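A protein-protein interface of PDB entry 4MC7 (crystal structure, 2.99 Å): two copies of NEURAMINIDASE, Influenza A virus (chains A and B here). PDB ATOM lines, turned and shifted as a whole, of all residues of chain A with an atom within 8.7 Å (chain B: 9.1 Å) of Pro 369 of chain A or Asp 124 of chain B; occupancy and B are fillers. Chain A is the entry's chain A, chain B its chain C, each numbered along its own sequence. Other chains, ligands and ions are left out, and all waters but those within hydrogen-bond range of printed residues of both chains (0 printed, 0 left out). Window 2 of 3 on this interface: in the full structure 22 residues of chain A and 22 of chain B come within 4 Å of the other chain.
The side-chain hydroxyl (OG1) of Thr 138 of chain B sits at hydrogen-bond distance from a ring nitrogen (NE2) of His 140 of chain B, 3.2 Å away. The side-chain hydroxyl (OH) of Tyr 313 of chain A lies within hydrogen-bond range of the backbone NH (N) of Met 368 of chain A, at 3.4 Å. NH2 of Arg 311 of chain A is in hydrogen-bond range of O of Met 368 of chain A (3.1 Å). O of Leu 315 of chain A is in hydrogen-bond range of N of Trp 373 of chain A, at 3.0 Å.
CZ of Phe 126 of chain B touches CE of Met 368 of chain A (3.6 Å). Met 368 of chain A touches His 140 of chain B (SD to CE1, 3.9 Å). OD2 of Asp 124 of chain B touches CG of Pro 369 of chain A, 3.7 Å away. CD of Pro 369 of chain A touches CE1 of His 140 of chain B, 3.95 Å away. CG1 of Val 371 of chain A touches CA of Gly 123 of chain B, at 3.3 Å. Asp 124 of chain B touches Val 371 of chain A (N to CG2, 3.5 Å). Trp 373 of chain A touches Ala 122 of chain B. Gly 123 of chain B touches Trp 373 of chain A. Trp 373 of chain A touches Phe 126 of chain B (CH2 to CE2, 3.6 Å).
Of chain B, only Phe 126 and His 140 come within 4 Å of Met 368 of chain A. Pro 369 of chain A touches just these residues of chain B: Asp 124 and His 140. Printed residues of chain B within 4 Å of Val 371 of chain A: Gly 123 and Asp 124. Printed residues of chain B within 4 Å of Trp 373 of chain A: Ala 122 (3.5 Å), Gly 123 (3.3 Å) and Phe 126 (3.6 Å). Val 121 of chain B touches none of the printed residues of chain A. Printed residues of chain A within 4 Å of Ala 122 of chain B: Trp 373. Gly 123 of chain B touches two residues of chain A. Of chain A, only Pro 369 (3.7 Å) and Val 371 (3.5 Å) come within 4 Å of Asp 124 of chain B. No residue of chain A comes within 4 Å of Gly 125 of chain B. Of the printed residues of chain A, Phe 126 of chain B touches Met 368 (3.6 Å) and Trp 373 (3.6 Å). Of the printed residues of chain A, His 140 of chain B touches Met 368 and Pro 369.
Of the 18 printed residues of chain A, 4 touch a printed residue of chain B. Printed residues of chain B that touch a printed residue of chain A: Ala 122, Gly 123, Asp 124, Phe 126 and His 140. Along chain B the printed residues that touch a printed residue of chain A span positions 122 to 140. Among the printed residues, no Asp or Glu carboxylate lies within 4 Å of a Lys or Arg side-chain nitrogen of the other chain.
No position is printed for both chains. Of the 9 pairs that touch across the chains among the printed residues, none has its exchanged pair printed and touching as well.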
ATOM      1  N   ASN A  24      28.239  22.056 -26.314  1.00  0.00           N
ATOM      2  CA  ASN A  24      28.720  21.522 -27.583  1.00  0.00           C
ATOM      3  C   ASN A  24      27.761  20.534 -28.228  1.00  0.00           C
ATOM      4  O   ASN A  24      28.004  20.078 -29.341  1.00  0.00           O
ATOM      5  CB  ASN A  24      30.114  20.922 -27.422  1.00  0.00           C
ATOM      6  CG  ASN A  24      31.159  21.979 -27.157  1.00  0.00           C
ATOM      7  OD1 ASN A  24      31.592  22.691 -28.072  1.00  0.00           O
ATOM      8  ND2 ASN A  24      31.558  22.107 -25.895  1.00  0.00           N
ATOM      9  N   GLY A  25      26.671  20.216 -27.527  1.00  0.00           N
ATOM     10  CA  GLY A  25      25.674  19.274 -28.017  1.00  0.00           C
ATOM     11  C   GLY A  25      24.321  19.406 -27.316  1.00  0.00           C
ATOM     12  O   GLY A  25      24.116  20.259 -26.446  1.00  0.00           O
ATOM     13  N   TRP A  26      23.367  18.574 -27.705  1.00  0.00           N
ATOM     14  CA  TRP A  26      22.049  18.650 -27.121  1.00  0.00           C
ATOM     15  C   TRP A  26      21.494  17.270 -26.909  1.00  0.00           C
ATOM     16  O   TRP A  26      21.516  16.393 -27.811  1.00  0.00           O
ATOM     17  CB  TRP A  26      21.121  19.446 -28.034  1.00  0.00           C
ATOM     18  CG  TRP A  26      21.629  20.840 -28.316  1.00  0.00           C
ATOM     19  CD1 TRP A  26      22.384  21.274 -29.406  1.00  0.00           C
ATOM     20  CD2 TRP A  26      21.459  22.027 -27.482  1.00  0.00           C
ATOM     21  NE1 TRP A  26      22.680  22.607 -29.306  1.00  0.00           N
ATOM     22  CE2 TRP A  26      22.160  23.121 -28.164  1.00  0.00           C
ATOM     23  CE3 TRP A  26      20.840  22.280 -26.289  1.00  0.00           C
ATOM     24  CZ2 TRP A  26      22.206  24.412 -27.638  1.00  0.00           C
ATOM     25  CZ3 TRP A  26      20.914  23.579 -25.769  1.00  0.00           C
ATOM     26  CH2 TRP A  26      21.583  24.614 -26.430  1.00  0.00           C
ATOM     27  N   VAL A  27      20.981  17.039 -25.707  1.00  0.00           N
ATOM     28  CA  VAL A  27      20.275  15.792 -25.453  1.00  0.00           C
ATOM     29  C   VAL A  27      18.885  16.076 -24.960  1.00  0.00           C
ATOM     30  O   VAL A  27      18.685  16.968 -24.131  1.00  0.00           O
ATOM     31  CB  VAL A  27      21.030  14.852 -24.494  1.00  0.00           C
ATOM     32  CG1 VAL A  27      22.528  15.080 -24.623  1.00  0.00           C
ATOM     33  CG2 VAL A  27      20.610  15.081 -23.101  1.00  0.00           C
ATOM     34  N   ARG A 311      29.331  23.223 -36.855  1.00  0.00           N
ATOM     35  CA  ARG A 311      28.650  21.945 -36.722  1.00  0.00           C
ATOM     36  C   ARG A 311      27.135  22.031 -36.796  1.00  0.00           C
ATOM     37  O   ARG A 311      26.493  22.761 -36.028  1.00  0.00           O
ATOM     38  CB  ARG A 311      29.024  21.295 -35.411  1.00  0.00           C
ATOM     39  CG  ARG A 311      28.303  19.990 -35.190  1.00  0.00           C
ATOM     40  CD  ARG A 311      28.954  18.944 -35.991  1.00  0.00           C
ATOM     41  NE  ARG A 311      28.396  17.615 -35.771  1.00  0.00           N
ATOM     42  CZ  ARG A 311      28.842  16.763 -34.855  1.00  0.00           C
ATOM     43  NH1 ARG A 311      29.827  17.130 -34.050  1.00  0.00           N
ATOM     44  NH2 ARG A 311      28.297  15.554 -34.735  1.00  0.00           N
ATOM     45  N   ASN A 312      26.559  21.258 -37.699  1.00  0.00           N
ATOM     46  CA  ASN A 312      25.116  21.245 -37.841  1.00  0.00           C
ATOM     47  C   ASN A 312      24.496  19.976 -37.263  1.00  0.00           C
ATOM     48  O   ASN A 312      24.770  18.872 -37.752  1.00  0.00           O
ATOM     49  CB  ASN A 312      24.762  21.382 -39.313  1.00  0.00           C
ATOM     50  CG  ASN A 312      23.327  21.081 -39.593  1.00  0.00           C
ATOM     51  OD1 ASN A 312      22.966  19.944 -39.949  1.00  0.00           O
ATOM     52  ND2 ASN A 312      22.482  22.089 -39.430  1.00  0.00           N
ATOM     53  N   TYR A 313      23.671  20.135 -36.227  1.00  0.00           N
ATOM     54  CA  TYR A 313      22.870  19.024 -35.683  1.00  0.00           C
ATOM     55  C   TYR A 313      21.443  19.011 -36.238  1.00  0.00           C
ATOM     56  O   TYR A 313      20.656  19.907 -35.986  1.00  0.00           O
ATOM     57  CB  TYR A 313      22.786  19.098 -34.156  1.00  0.00           C
ATOM     58  CG  TYR A 313      24.099  18.895 -33.443  1.00  0.00           C
ATOM     59  CD1 TYR A 313      24.815  19.980 -32.938  1.00  0.00           C
ATOM     60  CD2 TYR A 313      24.632  17.614 -33.272  1.00  0.00           C
ATOM     61  CE1 TYR A 313      26.019  19.790 -32.266  1.00  0.00           C
ATOM     62  CE2 TYR A 313      25.849  17.414 -32.615  1.00  0.00           C
ATOM     63  CZ  TYR A 313      26.537  18.500 -32.110  1.00  0.00           C
ATOM     64  OH  TYR A 313      27.732  18.280 -31.456  1.00  0.00           O
ATOM     65  N   GLN A 314      21.088  17.994 -36.984  1.00  0.00           N
ATOM     66  CA  GLN A 314      19.708  17.866 -37.405  1.00  0.00           C
ATOM     67  C   GLN A 314      18.982  17.050 -36.366  1.00  0.00           C
ATOM     68  O   GLN A 314      18.991  15.828 -36.420  1.00  0.00           O
ATOM     69  CB  GLN A 314      19.616  17.169 -38.764  1.00  0.00           C
ATOM     70  CG  GLN A 314      20.173  18.000 -39.891  1.00  0.00           C
ATOM     71  CD  GLN A 314      19.571  17.623 -41.203  1.00  0.00           C
ATOM     72  OE1 GLN A 314      18.671  16.641 -41.186  1.00  0.00           O
ATOM     73  NE2 GLN A 314      19.901  18.205 -42.229  1.00  0.00           N
ATOM     74  N   LEU A 315      18.342  17.717 -35.422  1.00  0.00           N
ATOM     75  CA  LEU A 315      17.752  17.002 -34.297  1.00  0.00           C
ATOM     76  C   LEU A 315      16.482  16.278 -34.634  1.00  0.00           C
ATOM     77  O   LEU A 315      16.238  15.192 -34.104  1.00  0.00           O
ATOM     78  CB  LEU A 315      17.496  17.943 -33.138  1.00  0.00           C
ATOM     79  CG  LEU A 315      18.733  18.602 -32.527  1.00  0.00           C
ATOM     80  CD1 LEU A 315      18.301  19.538 -31.406  1.00  0.00           C
ATOM     81  CD2 LEU A 315      19.692  17.549 -32.018  1.00  0.00           C
ATOM     82  N   THR A 364      24.801  19.855 -23.372  1.00  0.00           N
ATOM     83  CA  THR A 364      25.939  19.235 -22.712  1.00  0.00           C
ATOM     84  C   THR A 364      27.225  19.885 -23.219  1.00  0.00           C
ATOM     85  O   THR A 364      27.234  20.500 -24.313  1.00  0.00           O
ATOM     86  CB  THR A 364      25.967  17.683 -22.859  1.00  0.00           C
ATOM     87  OG1 THR A 364      27.007  17.131 -22.031  1.00  0.00           O
ATOM     88  CG2 THR A 364      26.195  17.279 -24.299  1.00  0.00           C
ATOM     89  N   GLY A 366      29.913  18.195 -23.766  1.00  0.00           N
ATOM     90  CA  GLY A 366      30.516  17.274 -24.715  1.00  0.00           C
ATOM     91  C   GLY A 366      29.970  17.458 -26.125  1.00  0.00           C
ATOM     92  O   GLY A 366      28.876  17.954 -26.340  1.00  0.00           O
ATOM     93  N   SER A 367      30.737  17.043 -27.110  1.00  0.00           N
ATOM     94  CA  SER A 367      30.172  16.931 -28.432  1.00  0.00           C
ATOM     95  C   SER A 367      29.285  15.698 -28.481  1.00  0.00           C
ATOM     96  O   SER A 367      29.434  14.756 -27.698  1.00  0.00           O
ATOM     97  CB  SER A 367      31.286  16.832 -29.461  1.00  0.00           C
ATOM     98  OG  SER A 367      30.738  16.735 -30.749  1.00  0.00           O
ATOM     99  N   MET A 368      28.364  15.691 -29.416  1.00  0.00           N
ATOM    100  CA  MET A 368      27.424  14.598 -29.498  1.00  0.00           C
ATOM    101  C   MET A 368      27.318  14.077 -30.902  1.00  0.00           C
ATOM    102  O   MET A 368      27.491  14.839 -31.853  1.00  0.00           O
ATOM    103  CB  MET A 368      26.065  15.070 -29.046  1.00  0.00           C
ATOM    104  CG  MET A 368      25.954  15.230 -27.538  1.00  0.00           C
ATOM    105  SD  MET A 368      25.278  13.768 -26.759  1.00  0.00           S
ATOM    106  CE  MET A 368      24.035  13.211 -27.921  1.00  0.00           C
ATOM    107  N   PRO A 369      27.024  12.773 -31.040  1.00  0.00           N
ATOM    108  CA  PRO A 369      26.888  12.130 -32.337  1.00  0.00           C
ATOM    109  C   PRO A 369      25.617  12.586 -33.062  1.00  0.00           C
ATOM    110  O   PRO A 369      24.734  13.195 -32.460  1.00  0.00           O
ATOM    111  CB  PRO A 369      26.758  10.654 -31.963  1.00  0.00           C
ATOM    112  CG  PRO A 369      26.050  10.690 -30.667  1.00  0.00           C
ATOM    113  CD  PRO A 369      26.682  11.845 -29.945  1.00  0.00           C
ATOM    114  N   ASP A 370      25.534  12.277 -34.351  1.00  0.00           N
ATOM    115  CA  ASP A 370      24.373  12.622 -35.153  1.00  0.00           C
ATOM    116  C   ASP A 370      23.228  11.710 -34.770  1.00  0.00           C
ATOM    117  O   ASP A 370      23.379  10.479 -34.759  1.00  0.00           O
ATOM    118  CB  ASP A 370      24.683  12.496 -36.644  1.00  0.00           C
ATOM    119  CG  ASP A 370      25.732  13.476 -37.096  1.00  0.00           C
ATOM    120  OD1 ASP A 370      25.813  14.580 -36.506  1.00  0.00           O
ATOM    121  OD2 ASP A 370      26.486  13.142 -38.039  1.00  0.00           O
ATOM    122  N   VAL A 371      22.091  12.315 -34.428  1.00  0.00           N
ATOM    123  CA  VAL A 371      20.912  11.544 -34.098  1.00  0.00           C
ATOM    124  C   VAL A 371      19.660  12.272 -34.571  1.00  0.00           C
ATOM    125  O   VAL A 371      19.502  13.487 -34.395  1.00  0.00           O
ATOM    126  CB  VAL A 371      20.781  11.308 -32.566  1.00  0.00           C
ATOM    127  CG1 VAL A 371      19.679  10.342 -32.290  1.00  0.00           C
ATOM    128  CG2 VAL A 371      22.084  10.823 -31.938  1.00  0.00           C
ATOM    129  N   ASN A 372      18.766  11.500 -35.169  1.00  0.00           N
ATOM    130  CA  ASN A 372      17.420  11.935 -35.465  1.00  0.00           C
ATOM    131  C   ASN A 372      16.497  11.394 -34.361  1.00  0.00           C
ATOM    132  O   ASN A 372      16.254  10.191 -34.306  1.00  0.00           O
ATOM    133  CB  ASN A 372      17.021  11.374 -36.838  1.00  0.00           C
ATOM    134  CG  ASN A 372      15.561  11.625 -37.192  1.00  0.00           C
ATOM    135  OD1 ASN A 372      14.757  12.149 -36.401  1.00  0.00           O
ATOM    136  ND2 ASN A 372      15.207  11.241 -38.403  1.00  0.00           N
ATOM    137  N   TRP A 373      15.987  12.271 -33.496  1.00  0.00           N
ATOM    138  CA  TRP A 373      15.014  11.900 -32.437  1.00  0.00           C
ATOM    139  C   TRP A 373      13.552  11.703 -32.850  1.00  0.00           C
ATOM    140  O   TRP A 373      13.092  12.166 -33.909  1.00  0.00           O
ATOM    141  CB  TRP A 373      15.095  12.901 -31.288  1.00  0.00           C
ATOM    142  CG  TRP A 373      16.488  13.014 -30.742  1.00  0.00           C
ATOM    143  CD1 TRP A 373      17.468  13.948 -31.068  1.00  0.00           C
ATOM    144  CD2 TRP A 373      17.126  12.124 -29.802  1.00  0.00           C
ATOM    145  NE1 TRP A 373      18.639  13.699 -30.386  1.00  0.00           N
ATOM    146  CE2 TRP A 373      18.503  12.623 -29.623  1.00  0.00           C
ATOM    147  CE3 TRP A 373      16.722  11.005 -29.108  1.00  0.00           C
ATOM    148  CZ2 TRP A 373      19.389  12.019 -28.767  1.00  0.00           C
ATOM    149  CZ3 TRP A 373      17.628  10.397 -28.248  1.00  0.00           C
ATOM    150  CH2 TRP A 373      18.925  10.895 -28.074  1.00  0.00           C
ATOM    151  N   GLU B  80      13.266   3.931 -31.246  1.00  0.00           N
ATOM    152  CA  GLU B  80      13.492   5.369 -31.236  1.00  0.00           C
ATOM    153  C   GLU B  80      12.321   6.138 -30.686  1.00  0.00           C
ATOM    154  O   GLU B  80      12.459   7.309 -30.344  1.00  0.00           O
ATOM    155  CB  GLU B  80      13.816   5.887 -32.638  1.00  0.00           C
ATOM    156  CG  GLU B  80      15.196   5.464 -33.152  1.00  0.00           C
ATOM    157  CD  GLU B  80      15.285   3.976 -33.483  1.00  0.00           C
ATOM    158  OE1 GLU B  80      14.232   3.347 -33.746  1.00  0.00           O
ATOM    159  OE2 GLU B  80      16.415   3.438 -33.481  1.00  0.00           O
ATOM    160  N   TRP B 105      15.192   3.368 -24.927  1.00  0.00           N
ATOM    161  CA  TRP B 105      14.511   2.111 -25.173  1.00  0.00           C
ATOM    162  C   TRP B 105      15.024   1.093 -24.215  1.00  0.00           C
ATOM    163  O   TRP B 105      14.584  -0.038 -24.216  1.00  0.00           O
ATOM    164  CB  TRP B 105      14.711   1.664 -26.632  1.00  0.00           C
ATOM    165  CG  TRP B 105      16.155   1.477 -27.038  1.00  0.00           C
ATOM    166  CD1 TRP B 105      17.025   0.438 -26.674  1.00  0.00           C
ATOM    167  CD2 TRP B 105      16.953   2.355 -27.898  1.00  0.00           C
ATOM    168  NE1 TRP B 105      18.263   0.618 -27.230  1.00  0.00           N
ATOM    169  CE2 TRP B 105      18.287   1.750 -27.983  1.00  0.00           C
ATOM    170  CE3 TRP B 105      16.712   3.540 -28.568  1.00  0.00           C
ATOM    171  CZ2 TRP B 105      19.309   2.327 -28.733  1.00  0.00           C
ATOM    172  CZ3 TRP B 105      17.754   4.114 -29.315  1.00  0.00           C
ATOM    173  CH2 TRP B 105      19.015   3.523 -29.395  1.00  0.00           C
ATOM    174  N   VAL B 121      19.373   4.329 -22.573  1.00  0.00           N
ATOM    175  CA  VAL B 121      20.024   4.197 -23.853  1.00  0.00           C
ATOM    176  C   VAL B 121      19.133   4.778 -24.909  1.00  0.00           C
ATOM    177  O   VAL B 121      18.028   4.283 -25.046  1.00  0.00           O
ATOM    178  CB  VAL B 121      20.187   2.734 -24.175  1.00  0.00           C
ATOM    179  CG1 VAL B 121      20.820   2.556 -25.531  1.00  0.00           C
ATOM    180  CG2 VAL B 121      21.046   2.085 -23.130  1.00  0.00           C
ATOM    181  N   ALA B 122      19.609   5.778 -25.665  1.00  0.00           N
ATOM    182  CA  ALA B 122      18.767   6.461 -26.656  1.00  0.00           C
ATOM    183  C   ALA B 122      19.475   6.802 -27.946  1.00  0.00           C
ATOM    184  O   ALA B 122      20.683   6.608 -28.058  1.00  0.00           O
ATOM    185  CB  ALA B 122      18.206   7.685 -26.071  1.00  0.00           C
ATOM    186  N   GLY B 123      18.692   7.301 -28.909  1.00  0.00           N
ATOM    187  CA  GLY B 123      19.153   7.759 -30.229  1.00  0.00           C
ATOM    188  C   GLY B 123      20.198   6.942 -30.969  1.00  0.00           C
ATOM    189  O   GLY B 123      19.899   5.871 -31.491  1.00  0.00           O
ATOM    190  N   ASP B 124      21.419   7.484 -31.031  1.00  0.00           N
ATOM    191  CA  ASP B 124      22.595   6.807 -31.588  1.00  0.00           C
ATOM    192  C   ASP B 124      22.749   5.391 -30.980  1.00  0.00           C
ATOM    193  O   ASP B 124      23.169   4.455 -31.651  1.00  0.00           O
ATOM    194  CB  ASP B 124      23.844   7.685 -31.327  1.00  0.00           C
ATOM    195  CG  ASP B 124      25.176   6.956 -31.584  1.00  0.00           C
ATOM    196  OD1 ASP B 124      25.328   6.350 -32.668  1.00  0.00           O
ATOM    197  OD2 ASP B 124      26.083   7.008 -30.709  1.00  0.00           O
ATOM    198  N   GLY B 125      22.364   5.236 -29.719  1.00  0.00           N
ATOM    199  CA  GLY B 125      22.658   4.039 -28.969  1.00  0.00           C
ATOM    200  C   GLY B 125      23.615   4.348 -27.826  1.00  0.00           C
ATOM    201  O   GLY B 125      24.330   3.451 -27.370  1.00  0.00           O
ATOM    202  N   PHE B 126      23.645   5.606 -27.368  1.00  0.00           N
ATOM    203  CA  PHE B 126      24.478   6.009 -26.217  1.00  0.00           C
ATOM    204  C   PHE B 126      23.662   6.009 -24.920  1.00  0.00           C
ATOM    205  O   PHE B 126      22.435   5.828 -24.920  1.00  0.00           O
ATOM    206  CB  PHE B 126      25.110   7.393 -26.431  1.00  0.00           C
ATOM    207  CG  PHE B 126      24.119   8.530 -26.351  1.00  0.00           C
ATOM    208  CD1 PHE B 126      24.066   9.342 -25.230  1.00  0.00           C
ATOM    209  CD2 PHE B 126      23.234   8.784 -27.407  1.00  0.00           C
ATOM    210  CE1 PHE B 126      23.147  10.372 -25.154  1.00  0.00           C
ATOM    211  CE2 PHE B 126      22.320   9.800 -27.339  1.00  0.00           C
ATOM    212  CZ  PHE B 126      22.273  10.600 -26.213  1.00  0.00           C
ATOM    213  N   VAL B 127      24.356   6.252 -23.821  1.00  0.00           N
ATOM    214  CA  VAL B 127      23.746   6.254 -22.519  1.00  0.00           C
ATOM    215  C   VAL B 127      23.736   7.654 -21.912  1.00  0.00           C
ATOM    216  O   VAL B 127      24.782   8.284 -21.759  1.00  0.00           O
ATOM    217  CB  VAL B 127      24.493   5.256 -21.595  1.00  0.00           C
ATOM    218  CG1 VAL B 127      24.369   5.630 -20.149  1.00  0.00           C
ATOM    219  CG2 VAL B 127      23.946   3.881 -21.772  1.00  0.00           C
ATOM    220  N   THR B 138      26.822  11.548 -19.789  1.00  0.00           N
ATOM    221  CA  THR B 138      26.590  10.654 -20.929  1.00  0.00           C
ATOM    222  C   THR B 138      27.785   9.727 -21.151  1.00  0.00           C
ATOM    223  O   THR B 138      28.954  10.083 -20.873  1.00  0.00           O
ATOM    224  CB  THR B 138      26.315  11.415 -22.247  1.00  0.00           C
ATOM    225  OG1 THR B 138      27.441  12.231 -22.560  1.00  0.00           O
ATOM    226  CG2 THR B 138      25.122  12.317 -22.119  1.00  0.00           C
ATOM    227  N   ILE B 139      27.474   8.537 -21.651  1.00  0.00           N
ATOM    228  CA  ILE B 139      28.474   7.530 -21.980  1.00  0.00           C
ATOM    229  C   ILE B 139      28.312   7.082 -23.445  1.00  0.00           C
ATOM    230  O   ILE B 139      27.207   6.777 -23.883  1.00  0.00           O
ATOM    231  CB  ILE B 139      28.339   6.323 -21.065  1.00  0.00           C
ATOM    232  CG1 ILE B 139      28.596   6.721 -19.618  1.00  0.00           C
ATOM    233  CG2 ILE B 139      29.296   5.224 -21.483  1.00  0.00           C
ATOM    234  CD1 ILE B 139      28.356   5.589 -18.657  1.00  0.00           C
ATOM    235  N   HIS B 140      29.413   7.046 -24.190  1.00  0.00           N
ATOM    236  CA  HIS B 140      29.364   6.756 -25.614  1.00  0.00           C
ATOM    237  C   HIS B 140      30.063   5.473 -25.979  1.00  0.00           C
ATOM    238  O   HIS B 140      31.043   5.086 -25.339  1.00  0.00           O
ATOM    239  CB  HIS B 140      29.940   7.925 -26.390  1.00  0.00           C
ATOM    240  CG  HIS B 140      29.244   9.214 -26.110  1.00  0.00           C
ATOM    241  ND1 HIS B 140      28.119   9.581 -26.748  1.00  0.00           N
ATOM    242  CD2 HIS B 140      29.538  10.226 -25.203  1.00  0.00           C
ATOM    243  CE1 HIS B 140      27.713  10.777 -26.281  1.00  0.00           C
ATOM    244  NE2 HIS B 140      28.581  11.168 -25.332  1.00  0.00           N
ATOM    245  N   PRO B 141      29.570   4.791 -27.025  1.00  0.00           N
ATOM    246  CA  PRO B 141      30.119   3.513 -27.450  1.00  0.00           C
ATOM    247  C   PRO B 141      31.476   3.668 -28.133  1.00  0.00           C
ATOM    248  O   PRO B 141      31.646   4.529 -29.009  1.00  0.00           O
ATOM    249  CB  PRO B 141      29.099   3.017 -28.483  1.00  0.00           C
ATOM    250  CG  PRO B 141      28.001   4.011 -28.512  1.00  0.00           C
ATOM    251  CD  PRO B 141      28.547   5.272 -27.967  1.00  0.00           C
ATOM    252  N   THR B 142      32.429   2.838 -27.723  1.00  0.00           N
ATOM    253  CA  THR B 142      33.726   2.743 -28.392  1.00  0.00           C
ATOM    254  C   THR B 142      33.669   1.557 -29.357  1.00  0.00           C
ATOM    255  O   THR B 142      33.825   1.709 -30.575  1.00  0.00           O
ATOM    256  CB  THR B 142      34.890   2.545 -27.382  1.00  0.00           C
ATOM    257  OG1 THR B 142      34.767   1.266 -26.745  1.00  0.00           O
ATOM    258  CG2 THR B 142      34.896   3.647 -26.316  1.00  0.00           C
ATOM    259  N   GLY B 144      31.638   0.161 -30.881  1.00  0.00           N
ATOM    260  CA  GLY B 144      30.634   0.285 -31.948  1.00  0.00           C
ATOM    261  C   GLY B 144      29.270  -0.257 -31.575  1.00  0.00           C
ATOM    262  O   GLY B 144      29.112  -0.895 -30.536  1.00  0.00           O
ATOM    263  N   GLY B 145      28.274  -0.005 -32.423  1.00  0.00           N
ATOM    264  CA  GLY B 145      26.928  -0.542 -32.198  1.00  0.00           C
ATOM    265  C   GLY B 145      26.406  -0.107 -30.847  1.00  0.00           C
ATOM    266  O   GLY B 145      27.168   0.426 -30.054  1.00  0.00           O
ATOM    267  N   PRO B 146      25.113  -0.353 -30.558  1.00  0.00           N
ATOM    268  CA  PRO B 146      24.447   0.304 -29.418  1.00  0.00           C
ATOM    269  C   PRO B 146      24.956  -0.245 -28.094  1.00  0.00           C
ATOM    270  O   PRO B 146      25.238  -1.427 -28.014  1.00  0.00           O
ATOM    271  CB  PRO B 146      22.985  -0.100 -29.600  1.00  0.00           C
ATOM    272  CG  PRO B 146      23.090  -1.480 -30.164  1.00  0.00           C
ATOM    273  CD  PRO B 146      24.304  -1.466 -31.084  1.00  0.00           C
ATOM    274  N   LEU B 147      25.092   0.593 -27.078  1.00  0.00           N
ATOM    275  CA  LEU B 147      25.301   0.084 -25.734  1.00  0.00           C
ATOM    276  C   LEU B 147      24.028  -0.537 -25.170  1.00  0.00           C
ATOM    277  O   LEU B 147      22.914  -0.418 -25.721  1.00  0.00           O
ATOM    278  CB  LEU B 147      25.757   1.176 -24.788  1.00  0.00           C
ATOM    279  CG  LEU B 147      26.981   1.976 -25.156  1.00  0.00           C
ATOM    280  CD1 LEU B 147      26.864   3.349 -24.525  1.00  0.00           C
ATOM    281  CD2 LEU B 147      28.120   1.282 -24.604  1.00  0.00           C
ATOM    282  N   ASP B 167      28.744  -3.360 -24.768  1.00  0.00           N
ATOM    283  CA  ASP B 167      29.072  -2.752 -26.057  1.00  0.00           C
ATOM    284  C   ASP B 167      29.257  -3.857 -27.114  1.00  0.00           C
ATOM    285  O   ASP B 167      29.531  -5.013 -26.785  1.00  0.00           O
ATOM    286  CB  ASP B 167      30.379  -1.956 -25.909  1.00  0.00           C
ATOM    287  CG  ASP B 167      30.501  -0.806 -26.906  1.00  0.00           C
ATOM    288  OD1 ASP B 167      29.683  -0.729 -27.840  1.00  0.00           O
ATOM    289  OD2 ASP B 167      31.424   0.031 -26.757  1.00  0.00           O
